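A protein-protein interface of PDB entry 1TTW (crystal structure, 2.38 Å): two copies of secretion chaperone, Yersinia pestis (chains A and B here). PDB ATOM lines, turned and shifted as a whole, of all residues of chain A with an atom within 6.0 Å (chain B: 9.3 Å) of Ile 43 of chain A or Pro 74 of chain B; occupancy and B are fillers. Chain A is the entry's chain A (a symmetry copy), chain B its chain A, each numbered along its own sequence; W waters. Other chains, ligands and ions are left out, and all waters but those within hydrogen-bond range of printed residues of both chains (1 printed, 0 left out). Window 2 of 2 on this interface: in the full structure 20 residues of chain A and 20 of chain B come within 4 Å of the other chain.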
ATOM      1  N   ALA A  41       6.622  -3.001  23.236  1.00  0.00           N
ATOM      2  CA  ALA A  41       7.195  -4.224  22.587  1.00  0.00           C
ATOM      3  C   ALA A  41       8.656  -4.370  22.959  1.00  0.00           C
ATOM      4  O   ALA A  41       9.435  -3.453  22.861  1.00  0.00           O
ATOM      5  CB  ALA A  41       6.966  -4.219  20.951  1.00  0.00           C
ATOM      6  N   PRO A  42       9.057  -5.548  23.312  1.00  0.00           N
ATOM      7  CA  PRO A  42      10.511  -5.866  23.456  1.00  0.00           C
ATOM      8  C   PRO A  42      11.143  -5.786  22.075  1.00  0.00           C
ATOM      9  O   PRO A  42      10.618  -6.090  20.998  1.00  0.00           O
ATOM     10  CB  PRO A  42      10.547  -7.289  23.744  1.00  0.00           C
ATOM     11  CG  PRO A  42       9.096  -7.789  23.645  1.00  0.00           C
ATOM     12  CD  PRO A  42       8.173  -6.695  23.248  1.00  0.00           C
ATOM     13  N   ILE A  43      12.303  -5.203  22.095  1.00  0.00           N
ATOM     14  CA  ILE A  43      12.973  -4.986  20.851  1.00  0.00           C
ATOM     15  C   ILE A  43      14.395  -5.649  20.610  1.00  0.00           C
ATOM     16  O   ILE A  43      14.832  -5.701  19.452  1.00  0.00           O
ATOM     17  CB  ILE A  43      12.961  -3.541  20.743  1.00  0.00           C
ATOM     18  CG1 ILE A  43      12.782  -3.090  19.328  1.00  0.00           C
ATOM     19  CG2 ILE A  43      14.292  -2.922  21.233  1.00  0.00           C
ATOM     20  CD1 ILE A  43      13.625  -1.816  19.297  1.00  0.00           C
ATOM     21  N   ASN A  44      15.020  -6.193  21.656  1.00  0.00           N
ATOM     22  CA  ASN A  44      16.508  -6.611  21.724  1.00  0.00           C
ATOM     23  C   ASN A  44      16.333  -7.587  22.780  1.00  0.00           C
ATOM     24  O   ASN A  44      15.339  -7.575  23.455  1.00  0.00           O
ATOM     25  CB  ASN A  44      17.357  -5.445  22.538  1.00  0.00           C
ATOM     26  CG  ASN A  44      17.767  -4.549  21.597  1.00  0.00           C
ATOM     27  OD1 ASN A  44      17.525  -4.889  20.379  1.00  0.00           O
ATOM     28  ND2 ASN A  44      18.403  -3.514  21.929  1.00  0.00           N
ATOM     29  N   GLU A  45      17.387  -8.051  23.265  1.00  0.00           N
ATOM     30  CA  GLU A  45      17.370  -8.794  24.500  1.00  0.00           C
ATOM     31  C   GLU A  45      17.334  -7.940  25.699  1.00  0.00           C
ATOM     32  O   GLU A  45      17.044  -8.414  26.811  1.00  0.00           O
ATOM     33  CB  GLU A  45      18.787  -9.542  24.563  1.00  0.00           C
ATOM     34  CG  GLU A  45      18.943 -10.581  23.456  1.00  0.00           C
ATOM     35  CD  GLU A  45      17.752 -11.611  23.541  1.00  0.00           C
ATOM     36  OE1 GLU A  45      17.777 -12.452  24.555  1.00  0.00           O
ATOM     37  OE2 GLU A  45      16.798 -11.569  22.639  1.00  0.00           O
ATOM     38  N   GLU A  47      16.063  -4.666  25.899  1.00  0.00           N
ATOM     39  CA  GLU A  47      15.227  -3.520  25.822  1.00  0.00           C
ATOM     40  C   GLU A  47      13.887  -3.499  25.132  1.00  0.00           C
ATOM     41  O   GLU A  47      13.530  -4.418  24.322  1.00  0.00           O
ATOM     42  CB  GLU A  47      16.112  -2.379  25.452  1.00  0.00           C
ATOM     43  CG  GLU A  47      16.206  -1.893  24.092  1.00  0.00           C
ATOM     44  CD  GLU A  47      17.593  -1.218  24.053  1.00  0.00           C
ATOM     45  OE1 GLU A  47      18.145  -1.226  25.189  1.00  0.00           O
ATOM     46  OE2 GLU A  47      18.121  -0.789  23.000  1.00  0.00           O
ATOM     47  N   LEU A  48      13.037  -2.523  25.599  1.00  0.00           N
ATOM     48  CA  LEU A  48      11.670  -2.383  25.032  1.00  0.00           C
ATOM     49  C   LEU A  48      11.470  -1.086  24.424  1.00  0.00           C
ATOM     50  O   LEU A  48      12.173  -0.059  24.713  1.00  0.00           O
ATOM     51  CB  LEU A  48      10.643  -2.676  26.054  1.00  0.00           C
ATOM     52  CG  LEU A  48      10.311  -1.757  27.284  1.00  0.00           C
ATOM     53  CD1 LEU A  48      10.003  -0.361  26.929  1.00  0.00           C
ATOM     54  CD2 LEU A  48       9.011  -2.163  27.683  1.00  0.00           C
ATOM     55  N   VAL A  49      10.428  -1.036  23.614  1.00  0.00           N
ATOM     56  CA  VAL A  49      10.043   0.184  23.012  1.00  0.00           C
ATOM     57  C   VAL A  49       8.600   0.494  23.486  1.00  0.00           C
ATOM     58  O   VAL A  49       7.797  -0.385  23.612  1.00  0.00           O
ATOM     59  CB  VAL A  49      10.311   0.035  21.510  1.00  0.00           C
ATOM     60  CG1 VAL A  49       9.273  -0.776  20.738  1.00  0.00           C
ATOM     61  CG2 VAL A  49      10.413   1.270  20.885  1.00  0.00           C
ATOM     62  N   GLN A  94      12.847   4.233  24.262  1.00  0.00           N
ATOM     63  CA  GLN A  94      13.363   2.795  24.305  1.00  0.00           C
ATOM     64  C   GLN A  94      14.004   2.721  25.572  1.00  0.00           C
ATOM     65  O   GLN A  94      14.772   3.653  25.822  1.00  0.00           O
ATOM     66  CB  GLN A  94      14.580   2.602  23.220  1.00  0.00           C
ATOM     67  CG  GLN A  94      14.957   1.170  22.707  1.00  0.00           C
ATOM     68  CD  GLN A  94      15.829   1.218  21.276  1.00  0.00           C
ATOM     69  OE1 GLN A  94      15.466   1.767  20.217  1.00  0.00           O
ATOM     70  NE2 GLN A  94      17.005   0.811  21.411  1.00  0.00           N
ATOM     71  N   LEU B  71      13.650   6.418  13.886  1.00  0.00           N
ATOM     72  CA  LEU B  71      12.891   5.408  14.497  1.00  0.00           C
ATOM     73  C   LEU B  71      13.770   4.673  15.397  1.00  0.00           C
ATOM     74  O   LEU B  71      14.986   4.981  15.465  1.00  0.00           O
ATOM     75  CB  LEU B  71      12.357   4.480  13.488  1.00  0.00           C
ATOM     76  CG  LEU B  71      10.853   4.275  13.320  1.00  0.00           C
ATOM     77  CD1 LEU B  71      10.405   2.812  12.718  1.00  0.00           C
ATOM     78  CD2 LEU B  71      10.134   4.505  14.666  1.00  0.00           C
ATOM     79  N   PHE B  72      13.172   3.831  16.224  1.00  0.00           N
ATOM     80  CA  PHE B  72      13.960   3.084  17.159  1.00  0.00           C
ATOM     81  C   PHE B  72      14.625   1.817  16.506  1.00  0.00           C
ATOM     82  O   PHE B  72      14.050   1.237  15.666  1.00  0.00           O
ATOM     83  CB  PHE B  72      13.011   2.540  18.256  1.00  0.00           C
ATOM     84  CG  PHE B  72      11.707   2.100  17.732  1.00  0.00           C
ATOM     85  CD1 PHE B  72      11.561   0.793  17.172  1.00  0.00           C
ATOM     86  CD2 PHE B  72      10.619   2.889  17.760  1.00  0.00           C
ATOM     87  CE1 PHE B  72      10.359   0.295  16.762  1.00  0.00           C
ATOM     88  CE2 PHE B  72       9.296   2.406  17.295  1.00  0.00           C
ATOM     89  CZ  PHE B  72       9.199   1.115  16.802  1.00  0.00           C
ATOM     90  N   SER B  73      15.670   1.255  17.099  1.00  0.00           N
ATOM     91  CA  SER B  73      16.272   0.143  16.554  1.00  0.00           C
ATOM     92  C   SER B  73      16.733  -0.753  17.580  1.00  0.00           C
ATOM     93  O   SER B  73      17.419  -0.397  18.608  1.00  0.00           O
ATOM     94  CB  SER B  73      17.494   0.589  15.779  1.00  0.00           C
ATOM     95  OG  SER B  73      18.202  -0.549  15.241  1.00  0.00           O
ATOM     96  N   PRO B  74      16.661  -1.982  17.171  1.00  0.00           N
ATOM     97  CA  PRO B  74      17.212  -3.115  17.974  1.00  0.00           C
ATOM     98  C   PRO B  74      18.714  -3.035  18.144  1.00  0.00           C
ATOM     99  O   PRO B  74      19.229  -3.469  19.162  1.00  0.00           O
ATOM    100  CB  PRO B  74      16.723  -4.386  17.258  1.00  0.00           C
ATOM    101  CG  PRO B  74      16.032  -4.016  16.054  1.00  0.00           C
ATOM    102  CD  PRO B  74      16.081  -2.431  15.886  1.00  0.00           C
ATOM    103  N   LEU B  75      19.369  -2.264  17.343  1.00  0.00           N
ATOM    104  CA  LEU B  75      20.790  -2.286  17.283  1.00  0.00           C
ATOM    105  C   LEU B  75      21.522  -1.095  17.809  1.00  0.00           C
ATOM    106  O   LEU B  75      21.117  -0.005  17.607  1.00  0.00           O
ATOM    107  CB  LEU B  75      21.204  -2.238  15.796  1.00  0.00           C
ATOM    108  CG  LEU B  75      21.282  -3.374  14.731  1.00  0.00           C
ATOM    109  CD1 LEU B  75      21.012  -4.710  15.046  1.00  0.00           C
ATOM    110  CD2 LEU B  75      20.401  -2.890  13.479  1.00  0.00           C
ATOM    111  N   SER B  76      22.747  -1.300  18.226  1.00  0.00           N
ATOM    112  CA  SER B  76      23.518  -0.278  18.863  1.00  0.00           C
ATOM    113  C   SER B  76      24.255   0.478  17.835  1.00  0.00           C
ATOM    114  O   SER B  76      24.342  -0.002  16.752  1.00  0.00           O
ATOM    115  CB  SER B  76      24.547  -0.928  19.655  1.00  0.00           C
ATOM    116  OG  SER B  76      23.891  -2.060  20.110  1.00  0.00           O
ATOM    117  N   GLY B  77      24.812   1.617  18.152  1.00  0.00           N
ATOM    118  CA  GLY B  77      25.497   2.326  17.123  1.00  0.00           C
ATOM    119  C   GLY B  77      24.745   3.055  16.081  1.00  0.00           C
ATOM    120  O   GLY B  77      25.344   3.695  15.190  1.00  0.00           O
ATOM    121  N   VAL B  78      23.451   3.106  16.181  1.00  0.00           N
ATOM    122  CA  VAL B  78      22.675   3.966  15.260  1.00  0.00           C
ATOM    123  C   VAL B  78      23.036   5.426  15.300  1.00  0.00           C
ATOM    124  O   VAL B  78      23.484   5.880  16.339  1.00  0.00           O
ATOM    125  CB  VAL B  78      21.151   3.836  15.535  1.00  0.00           C
ATOM    126  CG1 VAL B  78      20.419   4.219  14.297  1.00  0.00           C
ATOM    127  CG2 VAL B  78      20.792   2.450  15.877  1.00  0.00           C
ATOM    128  N   ARG B  80      22.313   9.449  14.842  1.00  0.00           N
ATOM    129  CA  ARG B  80      21.052  10.302  14.988  1.00  0.00           C
ATOM    130  C   ARG B  80      21.444  11.624  14.583  1.00  0.00           C
ATOM    131  O   ARG B  80      22.623  11.891  14.727  1.00  0.00           O
ATOM    132  CB  ARG B  80      20.537  10.302  16.426  1.00  0.00           C
ATOM    133  CG  ARG B  80      20.286   8.923  16.911  1.00  0.00           C
ATOM    134  CD  ARG B  80      19.065   8.342  16.261  1.00  0.00           C
ATOM    135  NE  ARG B  80      18.520   7.066  16.896  1.00  0.00           N
ATOM    136  CZ  ARG B  80      17.568   6.378  16.345  1.00  0.00           C
ATOM    137  NH1 ARG B  80      17.011   6.856  15.248  1.00  0.00           N
ATOM    138  NH2 ARG B  80      17.097   5.272  16.926  1.00  0.00           N
HETATM  139  O   HOH W   1      19.540   1.375  19.381  1.00  0.00           O
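The backbone carbonyl oxygen of Ser 73 of chain B is in hydrogen-bond range of the side-chain amide nitrogen of Gln 94 of chain A.
The backbone carbonyl oxygen (O) of Pro 74 of chain B sits close to the side-chain amide oxygen (OD1) of Asn 44 of chain A (2.5 Å).
The backbone NH (N) of Leu 75 of chain B lies within hydrogen-bond range of the side-chain hydroxyl (OG) of Ser 73 of chain B (3.0 Å).
The backbone carbonyl oxygen of Ala 41 of chain A lies within hydrogen-bond range of the backbone NH of Val 49 of chain A, at 2.7 Å.
ND2 of Asn 44 of chain A sits at hydrogen-bond distance from OE2 of Glu 47 of chain A (2.9 Å).
The side-chain carboxylate (OE2) of Glu 47 of chain A lies within hydrogen-bond range of the side-chain amide nitrogen (NE2) of Gln 94 of chain A (2.5 Å).
Among the printed residues, merely in contact across the chains: Ile 43 of chain A with Pro 74 of chain B (3.2 Å), Gln 94 of chain A with Phe 72 of chain B (3.2 Å), Val 49 of chain A with Phe 72 of chain B (3.5 Å), Ile 43 of chain A with Ser 73 of chain B (3.7 Å) and Ile 43 of chain A with Phe 72 of chain B (3.9 Å).
Of chain B, only Phe 72, Ser 73 and Pro 74 come within 4 Å of Ile 43 of chain A.
Pro 74 of chain B touches just these residues of chain A: Ile 43 (3.2 Å) and Asn 44 (2.5 Å).
No residue of chain B comes within 4 Å of Pro 42 of chain A.
Of chain B, only Pro 74 comes within 4 Å of Asn 44 of chain A.
Of the printed residues of chain B, Val 49 of chain A touches Phe 72.
Of the printed residues of chain A, Ser 73 of chain B touches Ile 43 (3.7 Å) and Gln 94 (3.1 Å).
Of the printed residues of chain B, Gln 94 of chain A touches Phe 72 and Ser 73.
Of the printed residues of chain A, Phe 72 of chain B touches Ile 43 (3.9 Å), Val 49 (3.5 Å) and Gln 94 (3.2 Å).
The nearest residue of chain B that does not touch Ile 43 of chain A is Leu 75 of chain B (6.1 Å).
The nearest residue of chain A that does not touch Pro 74 of chain B is Glu 47 of chain A (4.8 Å).
Of the 9 printed residues of chain A, 4 touch a printed residue of chain B.
Hydrophobic or aromatic side chains of chain B within 4 Å of the printed part of chain A: Phe 72 and Pro 74.
Along chain B the printed residues that touch a printed residue of chain A span positions 72 to 74.
Among the printed residues, no Asp or Glu carboxylate lies within 4 Å of a Lys or Arg side-chain nitrogen of the other chain.
No position is printed for both chains.
Of the 7 pairs that touch across the chains among the printed residues, none has its exchanged pair printed and touching as well.
Water W1 lies within hydrogen-bond range of O of Leu 75 of chain B, O of Ser 73 of chain B and NE2 of Gln 94 of chain A.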
